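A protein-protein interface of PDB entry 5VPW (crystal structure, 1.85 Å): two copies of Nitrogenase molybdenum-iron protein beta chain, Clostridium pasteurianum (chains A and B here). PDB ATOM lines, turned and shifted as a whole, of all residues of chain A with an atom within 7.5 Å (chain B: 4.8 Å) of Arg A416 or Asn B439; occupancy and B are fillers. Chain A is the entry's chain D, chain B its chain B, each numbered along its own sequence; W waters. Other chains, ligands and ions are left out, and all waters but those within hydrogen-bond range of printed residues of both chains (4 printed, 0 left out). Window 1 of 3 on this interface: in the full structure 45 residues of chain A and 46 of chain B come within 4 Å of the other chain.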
ATOM      1  N   ARG A  58      -0.289 -27.504 -18.294  1.00  0.00           N
ATOM      2  CA  ARG A  58       0.303 -27.817 -19.595  1.00  0.00           C
ATOM      3  C   ARG A  58       1.600 -27.057 -19.848  1.00  0.00           C
ATOM      4  O   ARG A  58       2.492 -27.561 -20.552  1.00  0.00           O
ATOM      5  CB  ARG A  58      -0.691 -27.572 -20.722  1.00  0.00           C
ATOM      6  CG  ARG A  58      -1.875 -28.573 -20.723  1.00  0.00           C
ATOM      7  CD  ARG A  58      -2.999 -28.152 -21.677  1.00  0.00           C
ATOM      8  NE  ARG A  58      -4.017 -29.195 -21.794  1.00  0.00           N
ATOM      9  CZ  ARG A  58      -5.254 -29.005 -22.254  1.00  0.00           C
ATOM     10  NH1 ARG A  58      -5.662 -27.789 -22.622  1.00  0.00           N
ATOM     11  NH2 ARG A  58      -6.136 -30.011 -22.266  1.00  0.00           N
ATOM     12  N   HIS A  59       1.701 -25.841 -19.305  1.00  0.00           N
ATOM     13  CA  HIS A  59       2.893 -25.001 -19.540  1.00  0.00           C
ATOM     14  C   HIS A  59       4.030 -25.391 -18.601  1.00  0.00           C
ATOM     15  O   HIS A  59       5.170 -25.560 -19.034  1.00  0.00           O
ATOM     16  CB  HIS A  59       2.553 -23.516 -19.399  1.00  0.00           C
ATOM     17  CG  HIS A  59       3.738 -22.626 -19.421  1.00  0.00           C
ATOM     18  ND1 HIS A  59       4.157 -21.995 -20.576  1.00  0.00           N
ATOM     19  CD2 HIS A  59       4.646 -22.313 -18.461  1.00  0.00           C
ATOM     20  CE1 HIS A  59       5.246 -21.288 -20.314  1.00  0.00           C
ATOM     21  NE2 HIS A  59       5.568 -21.462 -19.045  1.00  0.00           N
ATOM     22  N   PHE A  60       3.712 -25.545 -17.312  1.00  0.00           N
ATOM     23  CA  PHE A  60       4.755 -25.815 -16.315  1.00  0.00           C
ATOM     24  C   PHE A  60       5.023 -27.291 -15.991  1.00  0.00           C
ATOM     25  O   PHE A  60       6.018 -27.576 -15.359  1.00  0.00           O
ATOM     26  CB  PHE A  60       4.443 -25.064 -15.012  1.00  0.00           C
ATOM     27  CG  PHE A  60       4.595 -23.591 -15.138  1.00  0.00           C
ATOM     28  CD1 PHE A  60       5.865 -23.036 -15.197  1.00  0.00           C
ATOM     29  CD2 PHE A  60       3.475 -22.746 -15.242  1.00  0.00           C
ATOM     30  CE1 PHE A  60       6.029 -21.663 -15.348  1.00  0.00           C
ATOM     31  CE2 PHE A  60       3.650 -21.376 -15.365  1.00  0.00           C
ATOM     32  CZ  PHE A  60       4.928 -20.843 -15.436  1.00  0.00           C
ATOM     33  N   LYS A  61       4.208 -28.206 -16.515  1.00  0.00           N
ATOM     34  CA  LYS A  61       4.222 -29.622 -16.092  1.00  0.00           C
ATOM     35  C   LYS A  61       4.302 -29.729 -14.551  1.00  0.00           C
ATOM     36  O   LYS A  61       5.113 -30.485 -13.973  1.00  0.00           O
ATOM     37  CB  LYS A  61       5.369 -30.392 -16.791  1.00  0.00           C
ATOM     38  CG  LYS A  61       5.513 -30.143 -18.298  1.00  0.00           C
ATOM     39  CD  LYS A  61       4.278 -30.500 -19.117  1.00  0.00           C
ATOM     40  CE  LYS A  61       4.536 -30.445 -20.615  1.00  0.00           C
ATOM     41  NZ  LYS A  61       3.255 -30.257 -21.358  1.00  0.00           N
ATOM     42  N   THR A 393       3.813 -21.781 -28.307  1.00  0.00           N
ATOM     43  CA  THR A 393       3.619 -23.068 -28.972  1.00  0.00           C
ATOM     44  C   THR A 393       2.778 -22.967 -30.245  1.00  0.00           C
ATOM     45  O   THR A 393       3.037 -23.667 -31.211  1.00  0.00           O
ATOM     46  CB  THR A 393       2.984 -24.083 -27.979  1.00  0.00           C
ATOM     47  OG1 THR A 393       3.977 -24.452 -27.012  1.00  0.00           O
ATOM     48  CG2 THR A 393       2.502 -25.302 -28.699  1.00  0.00           C
ATOM     49  N   LYS A 396       3.915 -23.095 -33.992  1.00  0.00           N
ATOM     50  CA  LYS A 396       4.457 -24.299 -34.580  1.00  0.00           C
ATOM     51  C   LYS A 396       3.759 -24.704 -35.869  1.00  0.00           C
ATOM     52  O   LYS A 396       4.359 -25.363 -36.716  1.00  0.00           O
ATOM     53  CB  LYS A 396       4.402 -25.440 -33.558  1.00  0.00           C
ATOM     54  CG  LYS A 396       3.009 -26.003 -33.342  1.00  0.00           C
ATOM     55  CD  LYS A 396       2.935 -27.001 -32.185  1.00  0.00           C
ATOM     56  CE  LYS A 396       3.758 -28.240 -32.454  1.00  0.00           C
ATOM     57  NZ  LYS A 396       3.728 -29.102 -31.250  1.00  0.00           N
ATOM     58  N   PHE A 406      12.260 -22.035 -35.787  1.00  0.00           N
ATOM     59  CA  PHE A 406      11.224 -21.715 -34.792  1.00  0.00           C
ATOM     60  C   PHE A 406      11.777 -21.784 -33.375  1.00  0.00           C
ATOM     61  O   PHE A 406      12.340 -22.817 -32.961  1.00  0.00           O
ATOM     62  CB  PHE A 406      10.027 -22.690 -34.979  1.00  0.00           C
ATOM     63  CG  PHE A 406       8.928 -22.519 -33.974  1.00  0.00           C
ATOM     64  CD1 PHE A 406       8.452 -21.265 -33.660  1.00  0.00           C
ATOM     65  CD2 PHE A 406       8.342 -23.620 -33.357  1.00  0.00           C
ATOM     66  CE1 PHE A 406       7.429 -21.099 -32.762  1.00  0.00           C
ATOM     67  CE2 PHE A 406       7.305 -23.454 -32.458  1.00  0.00           C
ATOM     68  CZ  PHE A 406       6.841 -22.201 -32.172  1.00  0.00           C
ATOM     69  N   ARG A 408      10.614 -21.272 -29.447  1.00  0.00           N
ATOM     70  CA  ARG A 408       9.525 -21.148 -28.498  1.00  0.00           C
ATOM     71  C   ARG A 408       9.868 -20.124 -27.425  1.00  0.00           C
ATOM     72  O   ARG A 408      10.919 -20.198 -26.795  1.00  0.00           O
ATOM     73  CB  ARG A 408       9.239 -22.524 -27.851  1.00  0.00           C
ATOM     74  CG  ARG A 408       8.520 -23.502 -28.769  1.00  0.00           C
ATOM     75  CD  ARG A 408       8.681 -24.957 -28.307  1.00  0.00           C
ATOM     76  NE  ARG A 408       7.884 -25.785 -29.191  1.00  0.00           N
ATOM     77  CZ  ARG A 408       8.271 -26.266 -30.356  1.00  0.00           C
ATOM     78  NH1 ARG A 408       9.494 -26.039 -30.818  1.00  0.00           N
ATOM     79  NH2 ARG A 408       7.425 -26.991 -31.076  1.00  0.00           N
ATOM     80  N   ILE A 413       3.983 -22.417 -23.528  1.00  0.00           N
ATOM     81  CA  ILE A 413       4.823 -23.372 -24.201  1.00  0.00           C
ATOM     82  C   ILE A 413       4.442 -24.707 -23.536  1.00  0.00           C
ATOM     83  O   ILE A 413       4.746 -24.925 -22.355  1.00  0.00           O
ATOM     84  CB  ILE A 413       6.316 -23.073 -23.975  1.00  0.00           C
ATOM     85  CG1 ILE A 413       6.743 -21.722 -24.595  1.00  0.00           C
ATOM     86  CG2 ILE A 413       7.197 -24.167 -24.541  1.00  0.00           C
ATOM     87  CD1 ILE A 413       8.096 -21.245 -24.091  1.00  0.00           C
ATOM     88  N   MET A 414       3.755 -25.566 -24.292  1.00  0.00           N
ATOM     89  CA  MET A 414       3.114 -26.746 -23.765  1.00  0.00           C
ATOM     90  C   MET A 414       3.666 -28.049 -24.377  1.00  0.00           C
ATOM     91  O   MET A 414       3.208 -29.144 -24.038  1.00  0.00           O
ATOM     92  CB  MET A 414       1.595 -26.624 -24.004  1.00  0.00           C
ATOM     93  CG  MET A 414       0.998 -25.385 -23.361  1.00  0.00           C
ATOM     94  SD  MET A 414      -0.773 -25.261 -23.667  1.00  0.00           S
ATOM     95  CE  MET A 414      -0.808 -25.038 -25.413  1.00  0.00           C
ATOM     96  N   ASP A 415       4.670 -27.935 -25.252  1.00  0.00           N
ATOM     97  CA  ASP A 415       5.131 -29.047 -26.045  1.00  0.00           C
ATOM     98  C   ASP A 415       6.620 -29.348 -26.009  1.00  0.00           C
ATOM     99  O   ASP A 415       7.087 -30.139 -26.802  1.00  0.00           O
ATOM    100  CB  ASP A 415       4.649 -28.886 -27.499  1.00  0.00           C
ATOM    101  CG  ASP A 415       5.223 -27.642 -28.194  1.00  0.00           C
ATOM    102  OD1 ASP A 415       5.769 -26.704 -27.534  1.00  0.00           O
ATOM    103  OD2 ASP A 415       5.145 -27.639 -29.426  1.00  0.00           O
ATOM    104  N   ARG A 416       7.334 -28.743 -25.072  1.00  0.00           N
ATOM    105  CA  ARG A 416       8.741 -29.094 -24.764  1.00  0.00           C
ATOM    106  C   ARG A 416       8.877 -29.082 -23.252  1.00  0.00           C
ATOM    107  O   ARG A 416       8.000 -28.527 -22.546  1.00  0.00           O
ATOM    108  CB  ARG A 416       9.744 -28.135 -25.425  1.00  0.00           C
ATOM    109  CG  ARG A 416       9.718 -28.098 -26.944  1.00  0.00           C
ATOM    110  CD  ARG A 416      10.177 -29.427 -27.528  1.00  0.00           C
ATOM    111  NE  ARG A 416      10.327 -29.433 -28.983  1.00  0.00           N
ATOM    112  CZ  ARG A 416       9.385 -29.838 -29.841  1.00  0.00           C
ATOM    113  NH1 ARG A 416       8.164 -30.219 -29.419  1.00  0.00           N
ATOM    114  NH2 ARG A 416       9.666 -29.871 -31.131  1.00  0.00           N
ATOM    115  N   TYR A 417       9.958 -29.681 -22.759  1.00  0.00           N
ATOM    116  CA  TYR A 417      10.182 -29.920 -21.332  1.00  0.00           C
ATOM    117  C   TYR A 417      11.394 -29.154 -20.874  1.00  0.00           C
ATOM    118  O   TYR A 417      12.449 -29.195 -21.523  1.00  0.00           O
ATOM    119  CB  TYR A 417      10.378 -31.433 -21.015  1.00  0.00           C
ATOM    120  CG  TYR A 417       9.097 -32.211 -21.178  1.00  0.00           C
ATOM    121  CD1 TYR A 417       8.679 -32.627 -22.429  1.00  0.00           C
ATOM    122  CD2 TYR A 417       8.267 -32.477 -20.102  1.00  0.00           C
ATOM    123  CE1 TYR A 417       7.495 -33.290 -22.616  1.00  0.00           C
ATOM    124  CE2 TYR A 417       7.094 -33.182 -20.275  1.00  0.00           C
ATOM    125  CZ  TYR A 417       6.706 -33.580 -21.521  1.00  0.00           C
ATOM    126  OH  TYR A 417       5.495 -34.251 -21.713  1.00  0.00           O
ATOM    127  N   GLY A 418      11.244 -28.468 -19.747  1.00  0.00           N
ATOM    128  CA  GLY A 418      12.380 -27.791 -19.105  1.00  0.00           C
ATOM    129  C   GLY A 418      12.477 -26.284 -19.330  1.00  0.00           C
ATOM    130  O   GLY A 418      13.262 -25.603 -18.646  1.00  0.00           O
ATOM    131  N   HIS A 419      11.682 -25.733 -20.249  1.00  0.00           N
ATOM    132  CA  HIS A 419      11.774 -24.299 -20.544  1.00  0.00           C
ATOM    133  C   HIS A 419      11.642 -23.427 -19.287  1.00  0.00           C
ATOM    134  O   HIS A 419      12.264 -22.352 -19.200  1.00  0.00           O
ATOM    135  CB  HIS A 419      10.757 -23.842 -21.612  1.00  0.00           C
ATOM    136  CG  HIS A 419       9.349 -24.286 -21.331  1.00  0.00           C
ATOM    137  ND1 HIS A 419       8.445 -23.498 -20.655  1.00  0.00           N
ATOM    138  CD2 HIS A 419       8.696 -25.439 -21.631  1.00  0.00           C
ATOM    139  CE1 HIS A 419       7.288 -24.138 -20.561  1.00  0.00           C
ATOM    140  NE2 HIS A 419       7.418 -25.317 -21.137  1.00  0.00           N
ATOM    141  N   TYR A 420      10.838 -23.880 -18.314  1.00  0.00           N
ATOM    142  CA  TYR A 420      10.598 -23.162 -17.073  1.00  0.00           C
ATOM    143  C   TYR A 420      11.825 -23.187 -16.137  1.00  0.00           C
ATOM    144  O   TYR A 420      11.814 -22.523 -15.080  1.00  0.00           O
ATOM    145  CB  TYR A 420       9.354 -23.745 -16.327  1.00  0.00           C
ATOM    146  CG  TYR A 420       9.202 -25.209 -16.609  1.00  0.00           C
ATOM    147  CD1 TYR A 420       9.950 -26.138 -15.931  1.00  0.00           C
ATOM    148  CD2 TYR A 420       8.389 -25.649 -17.620  1.00  0.00           C
ATOM    149  CE1 TYR A 420       9.874 -27.478 -16.234  1.00  0.00           C
ATOM    150  CE2 TYR A 420       8.329 -26.984 -17.950  1.00  0.00           C
ATOM    151  CZ  TYR A 420       9.050 -27.895 -17.240  1.00  0.00           C
ATOM    152  OH  TYR A 420       9.007 -29.227 -17.579  1.00  0.00           O
ATOM    153  N   ASN A 422      14.776 -22.383 -17.720  1.00  0.00           N
ATOM    154  CA  ASN A 422      15.728 -21.658 -18.596  1.00  0.00           C
ATOM    155  C   ASN A 422      15.454 -20.128 -18.594  1.00  0.00           C
ATOM    156  O   ASN A 422      14.447 -19.673 -19.125  1.00  0.00           O
ATOM    157  CB  ASN A 422      15.623 -22.150 -20.042  1.00  0.00           C
ATOM    158  CG  ASN A 422      15.744 -23.667 -20.199  1.00  0.00           C
ATOM    159  OD1 ASN A 422      16.269 -24.395 -19.356  1.00  0.00           O
ATOM    160  ND2 ASN A 422      15.264 -24.137 -21.315  1.00  0.00           N
ATOM    161  N   GLU A 436      19.749 -20.625 -28.879  1.00  0.00           N
ATOM    162  CA  GLU A 436      18.541 -21.221 -29.459  1.00  0.00           C
ATOM    163  C   GLU A 436      18.326 -20.720 -30.852  1.00  0.00           C
ATOM    164  O   GLU A 436      18.024 -21.532 -31.735  1.00  0.00           O
ATOM    165  CB  GLU A 436      17.299 -20.902 -28.626  1.00  0.00           C
ATOM    166  CG  GLU A 436      17.104 -21.724 -27.342  1.00  0.00           C
ATOM    167  CD  GLU A 436      15.944 -21.188 -26.478  1.00  0.00           C
ATOM    168  OE1 GLU A 436      15.684 -19.962 -26.489  1.00  0.00           O
ATOM    169  OE2 GLU A 436      15.286 -21.978 -25.781  1.00  0.00           O
ATOM    170  N   VAL B 434      18.925 -33.516 -20.498  1.00  0.00           N
ATOM    171  CA  VAL B 434      17.559 -33.988 -20.710  1.00  0.00           C
ATOM    172  C   VAL B 434      16.753 -33.084 -21.650  1.00  0.00           C
ATOM    173  O   VAL B 434      15.969 -33.571 -22.477  1.00  0.00           O
ATOM    174  CB  VAL B 434      16.784 -34.178 -19.378  1.00  0.00           C
ATOM    175  CG1 VAL B 434      15.406 -34.754 -19.625  1.00  0.00           C
ATOM    176  CG2 VAL B 434      17.530 -35.121 -18.461  1.00  0.00           C
ATOM    177  N   GLU B 435      16.894 -31.782 -21.482  1.00  0.00           N
ATOM    178  CA  GLU B 435      16.305 -30.809 -22.426  1.00  0.00           C
ATOM    179  C   GLU B 435      16.743 -31.076 -23.872  1.00  0.00           C
ATOM    180  O   GLU B 435      15.879 -31.209 -24.751  1.00  0.00           O
ATOM    181  CB  GLU B 435      16.686 -29.382 -22.024  1.00  0.00           C
ATOM    182  CG  GLU B 435      16.015 -28.955 -20.747  1.00  0.00           C
ATOM    183  CD  GLU B 435      16.441 -27.579 -20.287  1.00  0.00           C
ATOM    184  OE1 GLU B 435      17.463 -27.059 -20.787  1.00  0.00           O
ATOM    185  OE2 GLU B 435      15.756 -27.044 -19.401  1.00  0.00           O
ATOM    186  N   GLU B 436      18.060 -31.164 -24.106  1.00  0.00           N
ATOM    187  CA  GLU B 436      18.609 -31.421 -25.445  1.00  0.00           C
ATOM    188  C   GLU B 436      18.121 -32.732 -26.034  1.00  0.00           C
ATOM    189  O   GLU B 436      17.680 -32.743 -27.206  1.00  0.00           O
ATOM    190  CB  GLU B 436      20.150 -31.428 -25.441  1.00  0.00           C
ATOM    191  CG  GLU B 436      20.799 -30.052 -25.241  1.00  0.00           C
ATOM    192  CD  GLU B 436      22.326 -30.108 -25.146  1.00  0.00           C
ATOM    193  OE1 GLU B 436      22.958 -29.066 -25.378  1.00  0.00           O
ATOM    194  OE2 GLU B 436      22.902 -31.179 -24.847  1.00  0.00           O
ATOM    195  N   ILE B 437      18.185 -33.831 -25.224  1.00  0.00           N
ATOM    196  CA  ILE B 437      17.733 -35.113 -25.677  1.00  0.00           C
ATOM    197  C   ILE B 437      16.237 -35.124 -26.060  1.00  0.00           C
ATOM    198  O   ILE B 437      15.846 -35.602 -27.132  1.00  0.00           O
ATOM    199  CB  ILE B 437      18.032 -36.174 -24.593  1.00  0.00           C
ATOM    200  CG1 ILE B 437      19.543 -36.364 -24.479  1.00  0.00           C
ATOM    201  CG2 ILE B 437      17.271 -37.481 -24.868  1.00  0.00           C
ATOM    202  CD1 ILE B 437      19.939 -37.250 -23.302  1.00  0.00           C
ATOM    203  N   THR B 438      15.386 -34.604 -25.191  1.00  0.00           N
ATOM    204  CA  THR B 438      13.949 -34.628 -25.452  1.00  0.00           C
ATOM    205  C   THR B 438      13.618 -33.663 -26.586  1.00  0.00           C
ATOM    206  O   THR B 438      12.765 -33.938 -27.447  1.00  0.00           O
ATOM    207  CB  THR B 438      13.108 -34.336 -24.186  1.00  0.00           C
ATOM    208  OG1 THR B 438      13.419 -33.047 -23.610  1.00  0.00           O
ATOM    209  CG2 THR B 438      13.373 -35.393 -23.167  1.00  0.00           C
ATOM    210  N   ASN B 439      14.289 -32.541 -26.604  1.00  0.00           N
ATOM    211  CA  ASN B 439      14.122 -31.623 -27.757  1.00  0.00           C
ATOM    212  C   ASN B 439      14.345 -32.285 -29.122  1.00  0.00           C
ATOM    213  O   ASN B 439      13.517 -32.123 -30.016  1.00  0.00           O
ATOM    214  CB  ASN B 439      15.010 -30.420 -27.651  1.00  0.00           C
ATOM    215  CG  ASN B 439      14.477 -29.378 -26.702  1.00  0.00           C
ATOM    216  OD1 ASN B 439      13.400 -29.510 -26.084  1.00  0.00           O
ATOM    217  ND2 ASN B 439      15.267 -28.347 -26.538  1.00  0.00           N
ATOM    218  N   VAL B 440      15.432 -33.039 -29.298  1.00  0.00           N
ATOM    219  CA  VAL B 440      15.713 -33.584 -30.631  1.00  0.00           C
ATOM    220  C   VAL B 440      14.802 -34.755 -30.930  1.00  0.00           C
ATOM    221  O   VAL B 440      14.440 -34.991 -32.106  1.00  0.00           O
ATOM    222  CB  VAL B 440      17.209 -33.937 -30.862  1.00  0.00           C
ATOM    223  CG1 VAL B 440      18.066 -32.682 -30.777  1.00  0.00           C
ATOM    224  CG2 VAL B 440      17.688 -34.997 -29.895  1.00  0.00           C
ATOM    225  N   ILE B 441      14.403 -35.494 -29.890  1.00  0.00           N
ATOM    226  CA  ILE B 441      13.455 -36.585 -30.066  1.00  0.00           C
ATOM    227  C   ILE B 441      12.101 -36.040 -30.498  1.00  0.00           C
ATOM    228  O   ILE B 441      11.515 -36.505 -31.508  1.00  0.00           O
ATOM    229  CB  ILE B 441      13.325 -37.452 -28.792  1.00  0.00           C
ATOM    230  CG1 ILE B 441      14.556 -38.348 -28.680  1.00  0.00           C
ATOM    231  CG2 ILE B 441      12.076 -38.317 -28.828  1.00  0.00           C
ATOM    232  CD1 ILE B 441      14.686 -39.063 -27.353  1.00  0.00           C
ATOM    233  N   LEU B 442      11.608 -35.067 -29.745  1.00  0.00           N
ATOM    234  CA  LEU B 442      10.352 -34.367 -30.115  1.00  0.00           C
ATOM    235  C   LEU B 442      10.387 -33.675 -31.492  1.00  0.00           C
ATOM    236  O   LEU B 442       9.385 -33.744 -32.267  1.00  0.00           O
ATOM    237  CB  LEU B 442       9.898 -33.395 -28.993  1.00  0.00           C
ATOM    238  CG  LEU B 442       9.462 -34.077 -27.684  1.00  0.00           C
ATOM    239  CD1 LEU B 442       9.382 -33.088 -26.530  1.00  0.00           C
ATOM    240  CD2 LEU B 442       8.115 -34.761 -27.785  1.00  0.00           C
ATOM    241  N   ASP B 443      11.531 -33.070 -31.846  1.00  0.00           N
ATOM    242  CA  ASP B 443      11.646 -32.389 -33.154  1.00  0.00           C
ATOM    243  C   ASP B 443      11.442 -33.371 -34.277  1.00  0.00           C
ATOM    244  O   ASP B 443      10.800 -33.044 -35.262  1.00  0.00           O
ATOM    245  CB  ASP B 443      13.011 -31.716 -33.336  1.00  0.00           C
ATOM    246  CG  ASP B 443      13.113 -30.381 -32.634  1.00  0.00           C
ATOM    247  OD1 ASP B 443      12.081 -29.823 -32.220  1.00  0.00           O
ATOM    248  OD2 ASP B 443      14.238 -29.866 -32.520  1.00  0.00           O
ATOM    249  N   GLU B 446       7.797 -34.494 -34.603  1.00  0.00           N
ATOM    250  CA  GLU B 446       6.980 -33.430 -35.254  1.00  0.00           C
ATOM    251  C   GLU B 446       7.310 -33.138 -36.714  1.00  0.00           C
ATOM    252  O   GLU B 446       6.445 -32.656 -37.454  1.00  0.00           O
ATOM    253  CB  GLU B 446       7.070 -32.106 -34.480  1.00  0.00           C
ATOM    254  CG  GLU B 446       6.621 -32.254 -33.041  1.00  0.00           C
ATOM    255  CD  GLU B 446       6.491 -30.934 -32.309  1.00  0.00           C
ATOM    256  OE1 GLU B 446       5.759 -30.931 -31.332  1.00  0.00           O
ATOM    257  OE2 GLU B 446       7.069 -29.911 -32.742  1.00  0.00           O
HETATM  258  O   HOH W   1      15.178 -26.286 -23.236  1.00  0.00           O
HETATM  259  O   HOH W   2      12.717 -28.535 -29.592  1.00  0.00           O
HETATM  260  O   HOH W   3      11.774 -31.064 -24.566  1.00  0.00           O
HETATM  261  O   HOH W   4      13.247 -28.124 -23.783  1.00  0.00           O
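Water W2 lies within hydrogen-bond range of the guanidinium group of Arg A416 and the side-chain carboxylate of Asp B443. Water W4 bridges the backbone carbonyl oxygen of Tyr A417 (2.6 Å) and the side-chain amide oxygen of Asn B439 (2.7 Å). Water W3 lies within hydrogen-bond range of OD1 of Asn B439, OG1 of Thr B438 and N of Tyr A417. Water W1 lies within hydrogen-bond range of ND2 of Asn A422 and OE1 of Glu B435.
Among the printed residues, pairs that only touch across the chains: Asp A415 with Leu B442 (3.7 Å), Asp A415 with Glu B446 (3.9 Å), Arg A416 with Asn B439 (3.5 Å), Arg A416 with Leu B442 (3.6 Å) and Tyr A417 with Glu B435 (3.7 Å).
O of Glu B435 sits close to OD1 of Asn B439 (3.3 Å). The side-chain amino group (NZ) of Lys A396 lies within salt-bridge range of the side-chain carboxylate (OD2) of Asp A415 (2.7 Å). The side-chain hydroxyl of Thr A393 lies within hydrogen-bond range of the side-chain carboxylate of Asp A415 (2.9 Å). The guanidinium group of Arg A408 is in salt-bridge range of the side-chain carboxylate of Asp A415 (2.8 Å). The side-chain amide oxygen of Asn A422 sits close to the backbone carbonyl oxygen of Gly A418. The backbone NH (N) of Gly A418 lies within hydrogen-bond range of the side-chain hydroxyl (OH) of Tyr A420 (3.2 Å).
Position printed for both chains: 436. Of the 11 pairs that touch across the chains among the printed residues, none has its exchanged pair printed and touching as well.
O of Gly A418 sits close to OE2 of Glu B435 (3.0 Å). The side-chain carboxylate of Glu B435 sits close to the side-chain amide oxygen of Asn A422 (2.7 Å). OE1 of Glu B446 is in salt-bridge range of NZ of Lys A396 (2.7 Å). NH2 of Arg A408 is in salt-bridge range of OE2 of Glu B446 (3.4 Å). OD1 of Asp B443 is in salt-bridge range of NH2 of Arg A416 (2.6 Å). OE2 of Glu B446 lies within salt-bridge range of NH2 of Arg A416, 3.1 Å away.
Arg A416 touches just these residues of chain B: Asn B439 (3.5 Å), Leu B442 (3.6 Å), Asp B443 (2.6 Å) and Glu B446 (3.1 Å). Of the printed residues of chain B, Gly A418 touches Glu B435 (3.0 Å). Tyr A420 touches none of the printed residues of chain B. Printed residues of chain B within 4 Å of Asn A422: Glu B435 (2.7 Å). Val B434 touches none of the printed residues of chain A. Of the printed residues of chain A, Glu B435 touches Tyr A417, Gly A418 and Asn A422. Of the printed residues of chain A, Asn B439 touches Arg A416 (3.5 Å). Of the printed residues of chain A, Asp B443 touches Arg A416 (2.6 Å). The nearest printed residue of chain B that does not touch Asp A415 is Asn B439 (6.4 Å).
Of the 11 printed residues of chain B, 5 touch a printed residue of chain A. Hydrophobic or aromatic side chains of chain B within 4 Å of the printed part of chain A: Leu B442. Of the 18 printed residues of chain A, 7 touch a printed residue of chain B. Printed residues of chain A that touch a printed residue of chain B: Lys A396, Arg A408, Asp A415, Arg A416, Tyr A417, Gly A418 and Asn A422. Among the printed residues, 11 pairs touch across the chains. Among the printed residues, Asp or Glu carboxylates within 4 Å of a Lys or Arg side-chain nitrogen of the other chain: Lys A396 with Glu B446 (2.7 Å), Arg A408 with Glu B446 (3.4 Å), Arg A416 with Asp B443 (2.6 Å) and Arg A416 with Glu B446 (3.1 Å).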
